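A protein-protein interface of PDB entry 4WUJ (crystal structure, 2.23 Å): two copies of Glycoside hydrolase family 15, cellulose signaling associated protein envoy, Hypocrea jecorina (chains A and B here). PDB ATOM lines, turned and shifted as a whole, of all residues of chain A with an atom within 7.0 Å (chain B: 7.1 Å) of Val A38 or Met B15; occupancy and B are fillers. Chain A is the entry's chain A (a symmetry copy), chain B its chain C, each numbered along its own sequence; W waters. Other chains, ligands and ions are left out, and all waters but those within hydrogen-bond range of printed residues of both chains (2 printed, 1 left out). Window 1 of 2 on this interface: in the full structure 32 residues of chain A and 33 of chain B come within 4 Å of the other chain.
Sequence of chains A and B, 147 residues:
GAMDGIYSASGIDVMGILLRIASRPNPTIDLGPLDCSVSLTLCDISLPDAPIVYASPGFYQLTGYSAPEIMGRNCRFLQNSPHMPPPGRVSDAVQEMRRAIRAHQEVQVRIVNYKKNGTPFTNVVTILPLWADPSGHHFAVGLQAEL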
ATOM      1  N   VAL A  14     -30.378 -18.279  12.466  1.00  0.00           N
ATOM      2  CA  VAL A  14     -30.286 -18.870  11.125  1.00  0.00           C
ATOM      3  C   VAL A  14     -29.613 -20.233  11.171  1.00  0.00           C
ATOM      4  O   VAL A  14     -30.026 -21.157  10.471  1.00  0.00           O
ATOM      5  CB  VAL A  14     -29.511 -17.982  10.105  1.00  0.00           C
ATOM      6  CG1 VAL A  14     -29.263 -18.769   8.849  1.00  0.00           C
ATOM      7  CG2 VAL A  14     -30.298 -16.758   9.737  1.00  0.00           C
ATOM      8  N   MET A  15     -28.565 -20.340  11.986  1.00  0.00           N
ATOM      9  CA  MET A  15     -27.921 -21.621  12.249  1.00  0.00           C
ATOM     10  C   MET A  15     -28.830 -22.780  12.706  1.00  0.00           C
ATOM     11  O   MET A  15     -28.632 -23.926  12.290  1.00  0.00           O
ATOM     12  CB  MET A  15     -26.784 -21.436  13.247  1.00  0.00           C
ATOM     13  CG  MET A  15     -25.447 -21.248  12.508  1.00  0.00           C
ATOM     14  SD  MET A  15     -24.133 -22.224  13.219  1.00  0.00           S
ATOM     15  CE  MET A  15     -23.483 -21.106  14.504  1.00  0.00           C
ATOM     16  N   LEU A  18     -30.063 -23.846   9.438  1.00  0.00           N
ATOM     17  CA  LEU A  18     -29.000 -24.627   8.819  1.00  0.00           C
ATOM     18  C   LEU A  18     -28.970 -26.059   9.350  1.00  0.00           C
ATOM     19  O   LEU A  18     -28.854 -27.027   8.577  1.00  0.00           O
ATOM     20  CB  LEU A  18     -27.634 -23.974   9.063  1.00  0.00           C
ATOM     21  CG  LEU A  18     -27.409 -22.558   8.512  1.00  0.00           C
ATOM     22  CD1 LEU A  18     -25.938 -22.183   8.667  1.00  0.00           C
ATOM     23  CD2 LEU A  18     -27.890 -22.396   7.037  1.00  0.00           C
ATOM     24  N   PRO A  33     -22.007 -24.997  -1.484  1.00  0.00           N
ATOM     25  CA  PRO A  33     -21.594 -24.094  -0.399  1.00  0.00           C
ATOM     26  C   PRO A  33     -22.453 -22.838  -0.298  1.00  0.00           C
ATOM     27  O   PRO A  33     -22.918 -22.321  -1.324  1.00  0.00           O
ATOM     28  CB  PRO A  33     -20.157 -23.727  -0.783  1.00  0.00           C
ATOM     29  CG  PRO A  33     -20.141 -23.811  -2.256  1.00  0.00           C
ATOM     30  CD  PRO A  33     -21.058 -24.966  -2.613  1.00  0.00           C
ATOM     31  N   LEU A  34     -22.685 -22.392   0.939  1.00  0.00           N
ATOM     32  CA  LEU A  34     -23.258 -21.082   1.226  1.00  0.00           C
ATOM     33  C   LEU A  34     -22.249 -20.222   1.951  1.00  0.00           C
ATOM     34  O   LEU A  34     -21.644 -20.671   2.947  1.00  0.00           O
ATOM     35  CB  LEU A  34     -24.447 -21.186   2.165  1.00  0.00           C
ATOM     36  CG  LEU A  34     -25.681 -21.976   1.744  1.00  0.00           C
ATOM     37  CD1 LEU A  34     -26.978 -21.392   2.353  1.00  0.00           C
ATOM     38  CD2 LEU A  34     -25.776 -22.023   0.306  1.00  0.00           C
ATOM     39  N   ASP A  35     -22.104 -18.974   1.520  1.00  0.00           N
ATOM     40  CA  ASP A  35     -21.395 -18.029   2.368  1.00  0.00           C
ATOM     41  C   ASP A  35     -22.320 -16.920   2.849  1.00  0.00           C
ATOM     42  O   ASP A  35     -23.514 -16.952   2.581  1.00  0.00           O
ATOM     43  CB  ASP A  35     -20.152 -17.483   1.688  1.00  0.00           C
ATOM     44  CG  ASP A  35     -20.470 -16.584   0.507  1.00  0.00           C
ATOM     45  OD1 ASP A  35     -21.619 -16.111   0.364  1.00  0.00           O
ATOM     46  OD2 ASP A  35     -19.523 -16.339  -0.275  1.00  0.00           O
ATOM     47  N   CYS A  36     -21.763 -15.971   3.590  1.00  0.00           N
ATOM     48  CA  CYS A  36     -22.575 -14.990   4.307  1.00  0.00           C
ATOM     49  C   CYS A  36     -23.182 -13.918   3.433  1.00  0.00           C
ATOM     50  O   CYS A  36     -23.989 -13.102   3.903  1.00  0.00           O
ATOM     51  CB  CYS A  36     -21.758 -14.338   5.410  1.00  0.00           C
ATOM     52  SG  CYS A  36     -21.246 -15.590   6.624  1.00  0.00           S
ATOM     53  N   SER A  37     -22.785 -13.916   2.169  1.00  0.00           N
ATOM     54  CA  SER A  37     -23.409 -13.030   1.185  1.00  0.00           C
ATOM     55  C   SER A  37     -24.646 -13.632   0.515  1.00  0.00           C
ATOM     56  O   SER A  37     -25.239 -12.985  -0.344  1.00  0.00           O
ATOM     57  CB  SER A  37     -22.397 -12.652   0.095  1.00  0.00           C
ATOM     58  OG  SER A  37     -21.729 -11.460   0.465  1.00  0.00           O
ATOM     59  N   VAL A  38     -24.980 -14.881   0.857  1.00  0.00           N
ATOM     60  CA  VAL A  38     -26.087 -15.586   0.228  1.00  0.00           C
ATOM     61  C   VAL A  38     -27.424 -14.819   0.410  1.00  0.00           C
ATOM     62  O   VAL A  38     -27.741 -14.296   1.485  1.00  0.00           O
ATOM     63  CB  VAL A  38     -26.248 -17.043   0.748  1.00  0.00           C
ATOM     64  CG1 VAL A  38     -26.780 -17.086   2.235  1.00  0.00           C
ATOM     65  CG2 VAL A  38     -27.206 -17.797  -0.172  1.00  0.00           C
ATOM     66  N   SER A  39     -28.177 -14.721  -0.685  1.00  0.00           N
ATOM     67  CA  SER A  39     -29.568 -14.321  -0.613  1.00  0.00           C
ATOM     68  C   SER A  39     -30.477 -15.423  -0.028  1.00  0.00           C
ATOM     69  O   SER A  39     -30.612 -16.506  -0.584  1.00  0.00           O
ATOM     70  CB  SER A  39     -30.070 -13.943  -2.010  1.00  0.00           C
ATOM     71  OG  SER A  39     -31.309 -13.305  -1.885  1.00  0.00           O
ATOM     72  N   LEU A  40     -31.149 -15.097   1.062  1.00  0.00           N
ATOM     73  CA  LEU A  40     -31.840 -16.072   1.879  1.00  0.00           C
ATOM     74  C   LEU A  40     -33.078 -15.410   2.490  1.00  0.00           C
ATOM     75  O   LEU A  40     -33.012 -14.284   3.031  1.00  0.00           O
ATOM     76  CB  LEU A  40     -30.899 -16.536   3.007  1.00  0.00           C
ATOM     77  CG  LEU A  40     -31.408 -17.713   3.818  1.00  0.00           C
ATOM     78  CD1 LEU A  40     -30.236 -18.518   4.406  1.00  0.00           C
ATOM     79  CD2 LEU A  40     -32.431 -17.254   4.901  1.00  0.00           C
ATOM     80  N   THR A  41     -34.219 -16.089   2.394  1.00  0.00           N
ATOM     81  CA  THR A  41     -35.401 -15.612   3.078  1.00  0.00           C
ATOM     82  C   THR A  41     -35.909 -16.726   3.969  1.00  0.00           C
ATOM     83  O   THR A  41     -35.746 -17.925   3.684  1.00  0.00           O
ATOM     84  CB  THR A  41     -36.525 -15.168   2.066  1.00  0.00           C
ATOM     85  OG1 THR A  41     -36.898 -16.277   1.245  1.00  0.00           O
ATOM     86  CG2 THR A  41     -36.048 -14.018   1.159  1.00  0.00           C
ATOM     87  N   ALA A  55     -34.846 -11.895   6.127  1.00  0.00           N
ATOM     88  CA  ALA A  55     -34.126 -11.841   4.873  1.00  0.00           C
ATOM     89  C   ALA A  55     -32.700 -11.441   5.191  1.00  0.00           C
ATOM     90  O   ALA A  55     -32.488 -10.569   6.034  1.00  0.00           O
ATOM     91  CB  ALA A  55     -34.781 -10.842   3.918  1.00  0.00           C
ATOM     92  N   SER A  56     -31.735 -12.075   4.513  1.00  0.00           N
ATOM     93  CA  SER A  56     -30.317 -11.827   4.756  1.00  0.00           C
ATOM     94  C   SER A  56     -29.896 -10.509   4.112  1.00  0.00           C
ATOM     95  O   SER A  56     -30.593  -9.986   3.269  1.00  0.00           O
ATOM     96  CB  SER A  56     -29.490 -12.966   4.221  1.00  0.00           C
ATOM     97  OG  SER A  56     -29.678 -13.081   2.827  1.00  0.00           O
ATOM     98  N   PRO A  57     -28.768  -9.949   4.547  1.00  0.00           N
ATOM     99  CA  PRO A  57     -28.197  -8.801   3.823  1.00  0.00           C
ATOM    100  C   PRO A  57     -28.025  -9.106   2.329  1.00  0.00           C
ATOM    101  O   PRO A  57     -28.154  -8.248   1.456  1.00  0.00           O
ATOM    102  CB  PRO A  57     -26.811  -8.620   4.478  1.00  0.00           C
ATOM    103  CG  PRO A  57     -26.962  -9.209   5.839  1.00  0.00           C
ATOM    104  CD  PRO A  57     -27.955 -10.349   5.706  1.00  0.00           C
ATOM    105  N   GLY A  58     -27.712 -10.350   2.028  1.00  0.00           N
ATOM    106  CA  GLY A  58     -27.486 -10.698   0.648  1.00  0.00           C
ATOM    107  C   GLY A  58     -28.754 -10.538  -0.190  1.00  0.00           C
ATOM    108  O   GLY A  58     -28.692 -10.173  -1.371  1.00  0.00           O
ATOM    109  N   PHE A  59     -29.909 -10.804   0.406  1.00  0.00           N
ATOM    110  CA  PHE A  59     -31.187 -10.638  -0.328  1.00  0.00           C
ATOM    111  C   PHE A  59     -31.453  -9.151  -0.628  1.00  0.00           C
ATOM    112  O   PHE A  59     -31.884  -8.796  -1.746  1.00  0.00           O
ATOM    113  CB  PHE A  59     -32.352 -11.240   0.463  1.00  0.00           C
ATOM    114  CG  PHE A  59     -33.738 -10.883  -0.075  1.00  0.00           C
ATOM    115  CD1 PHE A  59     -34.351  -9.698   0.299  1.00  0.00           C
ATOM    116  CD2 PHE A  59     -34.435 -11.768  -0.911  1.00  0.00           C
ATOM    117  CE1 PHE A  59     -35.617  -9.382  -0.173  1.00  0.00           C
ATOM    118  CE2 PHE A  59     -35.702 -11.475  -1.373  1.00  0.00           C
ATOM    119  CZ  PHE A  59     -36.299 -10.282  -1.010  1.00  0.00           C
ATOM    120  N   GLY A 142     -35.814 -19.973   1.622  1.00  0.00           N
ATOM    121  CA  GLY A 142     -35.580 -19.805   0.217  1.00  0.00           C
ATOM    122  C   GLY A 142     -34.226 -19.171  -0.013  1.00  0.00           C
ATOM    123  O   GLY A 142     -33.842 -18.222   0.647  1.00  0.00           O
ATOM    124  N   LEU A 143     -33.498 -19.712  -0.971  1.00  0.00           N
ATOM    125  CA  LEU A 143     -32.255 -19.137  -1.397  1.00  0.00           C
ATOM    126  C   LEU A 143     -32.423 -18.577  -2.818  1.00  0.00           C
ATOM    127  O   LEU A 143     -32.947 -19.255  -3.689  1.00  0.00           O
ATOM    128  CB  LEU A 143     -31.167 -20.209  -1.398  1.00  0.00           C
ATOM    129  CG  LEU A 143     -30.967 -20.953  -0.070  1.00  0.00           C
ATOM    130  CD1 LEU A 143     -29.908 -21.999  -0.271  1.00  0.00           C
ATOM    131  CD2 LEU A 143     -30.567 -20.000   1.072  1.00  0.00           C
ATOM    132  N   GLN A 144     -31.921 -17.362  -3.034  1.00  0.00           N
ATOM    133  CA  GLN A 144     -31.945 -16.701  -4.317  1.00  0.00           C
ATOM    134  C   GLN A 144     -30.515 -16.486  -4.851  1.00  0.00           C
ATOM    135  O   GLN A 144     -29.540 -16.354  -4.078  1.00  0.00           O
ATOM    136  CB  GLN A 144     -32.579 -15.317  -4.206  1.00  0.00           C
ATOM    137  CG  GLN A 144     -34.017 -15.238  -3.784  1.00  0.00           C
ATOM    138  CD  GLN A 144     -34.255 -15.507  -2.336  1.00  0.00           C
ATOM    139  OE1 GLN A 144     -33.410 -15.246  -1.454  1.00  0.00           O
ATOM    140  NE2 GLN A 144     -35.422 -16.046  -2.069  1.00  0.00           N
ATOM    141  N   ALA A 145     -30.416 -16.406  -6.179  1.00  0.00           N
ATOM    142  CA  ALA A 145     -29.153 -16.142  -6.857  1.00  0.00           C
ATOM    143  C   ALA A 145     -29.417 -15.639  -8.286  1.00  0.00           C
ATOM    144  O   ALA A 145     -30.225 -16.186  -9.043  1.00  0.00           O
ATOM    145  CB  ALA A 145     -28.248 -17.394  -6.862  1.00  0.00           C
ATOM    146  N   ILE B   6     -23.523 -21.549  -6.716  1.00  0.00           N
ATOM    147  CA  ILE B   6     -24.284 -20.312  -6.941  1.00  0.00           C
ATOM    148  C   ILE B   6     -24.648 -19.609  -5.625  1.00  0.00           C
ATOM    149  O   ILE B   6     -24.903 -18.419  -5.649  1.00  0.00           O
ATOM    150  CB  ILE B   6     -25.620 -20.467  -7.734  1.00  0.00           C
ATOM    151  CG1 ILE B   6     -26.650 -21.266  -6.918  1.00  0.00           C
ATOM    152  CG2 ILE B   6     -25.376 -21.052  -9.135  1.00  0.00           C
ATOM    153  CD1 ILE B   6     -28.022 -21.430  -7.630  1.00  0.00           C
ATOM    154  N   TYR B   7     -24.660 -20.308  -4.480  1.00  0.00           N
ATOM    155  CA  TYR B   7     -25.035 -19.596  -3.230  1.00  0.00           C
ATOM    156  C   TYR B   7     -23.820 -19.258  -2.370  1.00  0.00           C
ATOM    157  O   TYR B   7     -23.984 -18.878  -1.223  1.00  0.00           O
ATOM    158  CB  TYR B   7     -26.118 -20.356  -2.413  1.00  0.00           C
ATOM    159  CG  TYR B   7     -27.395 -20.581  -3.203  1.00  0.00           C
ATOM    160  CD1 TYR B   7     -28.119 -19.517  -3.725  1.00  0.00           C
ATOM    161  CD2 TYR B   7     -27.841 -21.857  -3.470  1.00  0.00           C
ATOM    162  CE1 TYR B   7     -29.300 -19.742  -4.459  1.00  0.00           C
ATOM    163  CE2 TYR B   7     -28.994 -22.082  -4.195  1.00  0.00           C
ATOM    164  CZ  TYR B   7     -29.717 -21.041  -4.691  1.00  0.00           C
ATOM    165  OH  TYR B   7     -30.877 -21.319  -5.436  1.00  0.00           O
ATOM    166  N   SER B   8     -22.609 -19.421  -2.929  1.00  0.00           N
ATOM    167  CA  SER B   8     -21.378 -18.888  -2.298  1.00  0.00           C
ATOM    168  C   SER B   8     -20.459 -18.238  -3.331  1.00  0.00           C
ATOM    169  O   SER B   8     -19.678 -18.921  -3.980  1.00  0.00           O
ATOM    170  CB  SER B   8     -20.607 -19.990  -1.587  1.00  0.00           C
ATOM    171  OG  SER B   8     -19.427 -19.469  -1.015  1.00  0.00           O
ATOM    172  N   ALA B   9     -20.566 -16.929  -3.501  1.00  0.00           N
ATOM    173  CA  ALA B   9     -19.719 -16.250  -4.474  1.00  0.00           C
ATOM    174  C   ALA B   9     -18.213 -16.409  -4.144  1.00  0.00           C
ATOM    175  O   ALA B   9     -17.370 -16.343  -5.046  1.00  0.00           O
ATOM    176  CB  ALA B   9     -20.078 -14.775  -4.560  1.00  0.00           C
ATOM    177  N   ILE B  12     -16.393 -20.582  -0.719  1.00  0.00           N
ATOM    178  CA  ILE B  12     -16.203 -21.158   0.591  1.00  0.00           C
ATOM    179  C   ILE B  12     -17.528 -21.488   1.223  1.00  0.00           C
ATOM    180  O   ILE B  12     -18.462 -20.697   1.157  1.00  0.00           O
ATOM    181  CB  ILE B  12     -15.492 -20.147   1.481  1.00  0.00           C
ATOM    182  CG1 ILE B  12     -14.038 -19.931   0.986  1.00  0.00           C
ATOM    183  CG2 ILE B  12     -15.509 -20.600   2.899  1.00  0.00           C
ATOM    184  CD1 ILE B  12     -13.382 -18.735   1.595  1.00  0.00           C
ATOM    185  N   ASP B  13     -17.608 -22.649   1.857  1.00  0.00           N
ATOM    186  CA  ASP B  13     -18.838 -23.069   2.514  1.00  0.00           C
ATOM    187  C   ASP B  13     -18.870 -22.573   3.950  1.00  0.00           C
ATOM    188  O   ASP B  13     -18.762 -23.351   4.894  1.00  0.00           O
ATOM    189  CB  ASP B  13     -18.989 -24.591   2.468  1.00  0.00           C
ATOM    190  CG  ASP B  13     -20.355 -25.059   2.988  1.00  0.00           C
ATOM    191  OD1 ASP B  13     -21.217 -24.195   3.228  1.00  0.00           O
ATOM    192  OD2 ASP B  13     -20.566 -26.283   3.147  1.00  0.00           O
ATOM    193  N   VAL B  14     -19.028 -21.270   4.111  1.00  0.00           N
ATOM    194  CA  VAL B  14     -18.982 -20.676   5.437  1.00  0.00           C
ATOM    195  C   VAL B  14     -20.023 -21.312   6.336  1.00  0.00           C
ATOM    196  O   VAL B  14     -19.782 -21.591   7.523  1.00  0.00           O
ATOM    197  CB  VAL B  14     -19.174 -19.147   5.394  1.00  0.00           C
ATOM    198  CG1 VAL B  14     -19.099 -18.540   6.767  1.00  0.00           C
ATOM    199  CG2 VAL B  14     -18.107 -18.509   4.486  1.00  0.00           C
ATOM    200  N   MET B  15     -21.189 -21.579   5.786  1.00  0.00           N
ATOM    201  CA  MET B  15     -22.254 -21.980   6.659  1.00  0.00           C
ATOM    202  C   MET B  15     -22.054 -23.459   7.025  1.00  0.00           C
ATOM    203  O   MET B  15     -22.357 -23.857   8.160  1.00  0.00           O
ATOM    204  CB  MET B  15     -23.618 -21.599   6.061  1.00  0.00           C
ATOM    205  CG  MET B  15     -23.648 -20.113   5.483  1.00  0.00           C
ATOM    206  SD  MET B  15     -24.214 -18.744   6.564  1.00  0.00           S
ATOM    207  CE  MET B  15     -25.716 -18.215   5.746  1.00  0.00           C
ATOM    208  N   GLY B  16     -21.467 -24.255   6.126  1.00  0.00           N
ATOM    209  CA  GLY B  16     -21.061 -25.610   6.494  1.00  0.00           C
ATOM    210  C   GLY B  16     -19.955 -25.633   7.589  1.00  0.00           C
ATOM    211  O   GLY B  16     -19.883 -26.532   8.445  1.00  0.00           O
ATOM    212  N   ILE B  17     -19.069 -24.643   7.525  1.00  0.00           N
ATOM    213  CA  ILE B  17     -18.099 -24.369   8.586  1.00  0.00           C
ATOM    214  C   ILE B  17     -18.801 -24.052   9.915  1.00  0.00           C
ATOM    215  O   ILE B  17     -18.500 -24.661  10.940  1.00  0.00           O
ATOM    216  CB  ILE B  17     -17.190 -23.213   8.154  1.00  0.00           C
ATOM    217  CG1 ILE B  17     -16.118 -23.756   7.210  1.00  0.00           C
ATOM    218  CG2 ILE B  17     -16.598 -22.488   9.332  1.00  0.00           C
ATOM    219  CD1 ILE B  17     -15.249 -22.711   6.624  1.00  0.00           C
ATOM    220  N   LEU B  18     -19.734 -23.111   9.894  1.00  0.00           N
ATOM    221  CA  LEU B  18     -20.499 -22.755  11.099  1.00  0.00           C
ATOM    222  C   LEU B  18     -21.291 -23.927  11.665  1.00  0.00           C
ATOM    223  O   LEU B  18     -21.352 -24.152  12.853  1.00  0.00           O
ATOM    224  CB  LEU B  18     -21.472 -21.618  10.791  1.00  0.00           C
ATOM    225  CG  LEU B  18     -20.757 -20.309  10.513  1.00  0.00           C
ATOM    226  CD1 LEU B  18     -21.725 -19.273  10.077  1.00  0.00           C
ATOM    227  CD2 LEU B  18     -19.974 -19.823  11.747  1.00  0.00           C
ATOM    228  N   LEU B  19     -21.914 -24.686  10.808  1.00  0.00           N
ATOM    229  CA  LEU B  19     -22.672 -25.793  11.298  1.00  0.00           C
ATOM    230  C   LEU B  19     -21.780 -26.800  12.031  1.00  0.00           C
ATOM    231  O   LEU B  19     -22.154 -27.300  13.088  1.00  0.00           O
ATOM    232  CB  LEU B  19     -23.399 -26.449  10.149  1.00  0.00           C
ATOM    233  CG  LEU B  19     -24.529 -27.379  10.547  1.00  0.00           C
ATOM    234  CD1 LEU B  19     -25.475 -26.707  11.557  1.00  0.00           C
ATOM    235  CD2 LEU B  19     -25.261 -27.814   9.268  1.00  0.00           C
ATOM    236  N   ARG B  20     -20.615 -27.124  11.475  1.00  0.00           N
ATOM    237  CA  ARG B  20     -19.714 -28.072  12.140  1.00  0.00           C
ATOM    238  C   ARG B  20     -19.341 -27.542  13.531  1.00  0.00           C
ATOM    239  O   ARG B  20     -19.317 -28.284  14.542  1.00  0.00           O
ATOM    240  CB  ARG B  20     -18.457 -28.284  11.308  1.00  0.00           C
ATOM    241  CG  ARG B  20     -18.382 -29.629  10.625  1.00  0.00           C
ATOM    242  CD  ARG B  20     -17.528 -29.563   9.360  1.00  0.00           C
ATOM    243  NE  ARG B  20     -16.235 -28.907   9.572  1.00  0.00           N
ATOM    244  CZ  ARG B  20     -15.576 -28.239   8.626  1.00  0.00           C
ATOM    245  NH1 ARG B  20     -16.087 -28.135   7.396  1.00  0.00           N
ATOM    246  NH2 ARG B  20     -14.405 -27.680   8.907  1.00  0.00           N
ATOM    247  N   ILE B  21     -19.066 -26.244  13.562  1.00  0.00           N
ATOM    248  CA  ILE B  21     -18.755 -25.556  14.796  1.00  0.00           C
ATOM    249  C   ILE B  21     -19.880 -25.670  15.804  1.00  0.00           C
ATOM    250  O   ILE B  21     -19.645 -25.966  16.975  1.00  0.00           O
ATOM    251  CB  ILE B  21     -18.451 -24.081  14.541  1.00  0.00           C
ATOM    252  CG1 ILE B  21     -16.975 -23.957  14.137  1.00  0.00           C
ATOM    253  CG2 ILE B  21     -18.731 -23.256  15.793  1.00  0.00           C
ATOM    254  CD1 ILE B  21     -16.661 -22.748  13.274  1.00  0.00           C
ATOM    255  N   ASP B  35     -27.210 -14.975  12.967  1.00  0.00           N
ATOM    256  CA  ASP B  35     -27.858 -14.722  11.665  1.00  0.00           C
ATOM    257  C   ASP B  35     -26.840 -14.243  10.542  1.00  0.00           C
ATOM    258  O   ASP B  35     -25.622 -14.182  10.784  1.00  0.00           O
ATOM    259  CB  ASP B  35     -29.074 -13.802  11.851  1.00  0.00           C
ATOM    260  CG  ASP B  35     -28.703 -12.342  12.064  1.00  0.00           C
ATOM    261  OD1 ASP B  35     -27.512 -11.967  11.931  1.00  0.00           O
ATOM    262  OD2 ASP B  35     -29.621 -11.547  12.392  1.00  0.00           O
ATOM    263  N   CYS B  36     -27.319 -13.935   9.326  1.00  0.00           N
ATOM    264  CA  CYS B  36     -26.397 -13.702   8.183  1.00  0.00           C
ATOM    265  C   CYS B  36     -25.749 -12.355   8.160  1.00  0.00           C
ATOM    266  O   CYS B  36     -24.959 -12.031   7.256  1.00  0.00           O
ATOM    267  CB  CYS B  36     -27.149 -13.892   6.855  1.00  0.00           C
ATOM    268  SG  CYS B  36     -27.746 -15.488   6.738  1.00  0.00           S
ATOM    269  N   VAL B  38     -24.004 -11.538  10.905  1.00  0.00           N
ATOM    270  CA  VAL B  38     -22.924 -11.688  11.880  1.00  0.00           C
ATOM    271  C   VAL B  38     -21.586 -11.233  11.260  1.00  0.00           C
ATOM    272  O   VAL B  38     -21.329 -11.465  10.091  1.00  0.00           O
ATOM    273  CB  VAL B  38     -22.779 -13.149  12.409  1.00  0.00           C
ATOM    274  CG1 VAL B  38     -22.295 -14.083  11.342  1.00  0.00           C
ATOM    275  CG2 VAL B  38     -21.788 -13.211  13.577  1.00  0.00           C
ATOM    276  N   TYR B  54     -11.337 -14.678   4.193  1.00  0.00           N
ATOM    277  CA  TYR B  54     -12.742 -14.340   4.013  1.00  0.00           C
ATOM    278  C   TYR B  54     -13.237 -13.487   5.170  1.00  0.00           C
ATOM    279  O   TYR B  54     -13.010 -13.845   6.346  1.00  0.00           O
ATOM    280  CB  TYR B  54     -13.590 -15.628   3.957  1.00  0.00           C
ATOM    281  CG  TYR B  54     -15.068 -15.367   3.870  1.00  0.00           C
ATOM    282  CD1 TYR B  54     -15.857 -15.209   5.021  1.00  0.00           C
ATOM    283  CD2 TYR B  54     -15.698 -15.251   2.619  1.00  0.00           C
ATOM    284  CE1 TYR B  54     -17.240 -14.959   4.920  1.00  0.00           C
ATOM    285  CE2 TYR B  54     -17.057 -15.013   2.519  1.00  0.00           C
ATOM    286  CZ  TYR B  54     -17.822 -14.849   3.661  1.00  0.00           C
ATOM    287  OH  TYR B  54     -19.161 -14.588   3.485  1.00  0.00           O
ATOM    288  N   PRO B  57     -20.142  -9.911   4.917  1.00  0.00           N
ATOM    289  CA  PRO B  57     -20.748  -8.567   4.839  1.00  0.00           C
ATOM    290  C   PRO B  57     -20.860  -7.864   6.218  1.00  0.00           C
ATOM    291  O   PRO B  57     -20.579  -6.677   6.371  1.00  0.00           O
ATOM    292  CB  PRO B  57     -22.164  -8.845   4.252  1.00  0.00           C
ATOM    293  CG  PRO B  57     -21.940 -10.142   3.424  1.00  0.00           C
ATOM    294  CD  PRO B  57     -20.955 -10.946   4.246  1.00  0.00           C
HETATM  295  O   HOH W   1     -22.544 -15.444  -2.059  1.00  0.00           O
HETATM  296  O   HOH W   2     -24.039 -23.121  -3.773  1.00  0.00           O
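Of the printed residues of chain B, Met A15 touches Leu B18 (3.4 Å).
Val A38 touches just these residues of chain B: Tyr B7 and Met B15.
Printed residues of chain A within 4 Å of Ser B8: Pro A33, Leu A34 and Asp A35.
Printed residues of chain A within 4 Å of Ala B9: Asp A35.
Of chain A, only Leu A18 (3.5 Å), Leu A34 (3.0 Å) and Val A38 (3.8 Å) come within 4 Å of Met B15.
Ile B21 touches none of the printed residues of chain A.
The nearest residue of chain A that does not touch Met B15 is Asp A35 (4.1 Å).
Water W1 bridges OD1 of Asp A35 (2.7 Å) and N of Ala B9 (2.9 Å).
Water W2 lies within hydrogen-bond range of the backbone carbonyl oxygen (O) of Pro A33 (2.8 Å), the backbone NH (N) of Tyr B7 (3.0 Å) and the backbone NH (N) of Ile B6 (3.4 Å).
Met A15 touches Leu B18, and with the chains exchanged Leu A18 touches Met B15.
Cys A36 touches Val B14, but with the chains exchanged Val A14 does not touch Cys B36 (4.1 Å).
Cys A36 touches Pro B57, and with the chains exchanged Pro A57 touches Cys B36.
OG of Ser A56 is in hydrogen-bond range of O of Val A38.
The backbone carbonyl oxygen (O) of Leu A40 lies within hydrogen-bond range of the backbone NH (N) of Ser A56, 3.0 Å away.
The side-chain carboxylate of Asp B13 sits at hydrogen-bond distance from the backbone NH of Gly B16, at 2.9 Å.
Of the 19 printed residues of chain B, 14 touch a printed residue of chain A.
Printed residues of chain B that touch a printed residue of chain A: Ile B6, Tyr B7, Ser B8, Ala B9, Ile B12, Asp B13, Val B14, Met B15, Leu B18, Leu B19, Asp B35, Cys B36, Tyr B54 and Pro B57.
Hydrophobic or aromatic side chains of chain A within 4 Å of the printed part of chain B: Val A14, Met A15, Leu A18, Pro A33, Leu A34, Val A38, Pro A57, Leu A143 and Ala A145.
Among the printed residues, no Asp or Glu carboxylate lies within 4 Å of a Lys or Arg side-chain nitrogen of the other chain.
The backbone carbonyl oxygen (O) of Leu A143 sits at hydrogen-bond distance from the side-chain hydroxyl (OH) of Tyr B7 (3.4 Å).
The backbone carbonyl oxygen (O) of Leu B18 sits close to the side-chain sulfur (SD) of Met A15, 3.4 Å away.
The side-chain carboxylate of Asp A35 lies within hydrogen-bond range of the side-chain hydroxyl of Ser B8, 3.2 Å away.
N of Ser B8 sits close to O of Pro A33 (3.3 Å).
The side-chain hydroxyl of Tyr B54 sits at hydrogen-bond distance from the backbone NH of Cys A36, 2.9 Å away.
N of Val B14 lies within hydrogen-bond range of O of Leu A34 (2.9 Å).
The backbone NH of Met B15 lies within hydrogen-bond range of the backbone carbonyl oxygen of Leu A34 (3.0 Å).
OD2 of Asp A35 sits at hydrogen-bond distance from N of Ala B9 (3.4 Å).
OD1 of Asp B13 sits at hydrogen-bond distance from N of Leu A34 (3.3 Å).
The backbone carbonyl oxygen (O) of Tyr B7 lies within hydrogen-bond range of the backbone NH (N) of Asp A35, at 3.3 Å.
Among the printed residues, merely in contact across the chains: Val A14 with Asp B35 (3.7 Å), Leu A18 with Met B15 (3.5 Å), Leu A18 with Leu B19 (3.7 Å), Pro A33 with Tyr B7 (3.4 Å), Pro A33 with Ile B12 (3.98 Å), Pro A33 with Asp B13 (3.6 Å), Leu A34 with Tyr B7 (3.2 Å), Leu A34 with Ser B8 (3.9 Å), Leu A34 with Ile B12 (3.7 Å), Asp A35 with Ile B12 (3.7 Å), Asp A35 with Val B14 (3.6 Å), Asp A35 with Tyr B54 (3.5 Å), Cys A36 with Val B14 (3.7 Å), Cys A36 with Cys B36 (3.7 Å), Cys A36 with Pro B57 (3.6 Å), Ser A37 with Tyr B54 (3.9 Å), Ser A37 with Pro B57 (3.2 Å), Val A38 with Tyr B7 (3.5 Å), Val A38 with Met B15 (3.8 Å), Ser A56 with Cys B36 (3.6 Å), Pro A57 with Cys B36 (3.7 Å), Gln A144 with Tyr B7 (3.4 Å), Ala A145 with Ile B6 (3.7 Å) and Ala A145 with Tyr B7 (3.5 Å).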
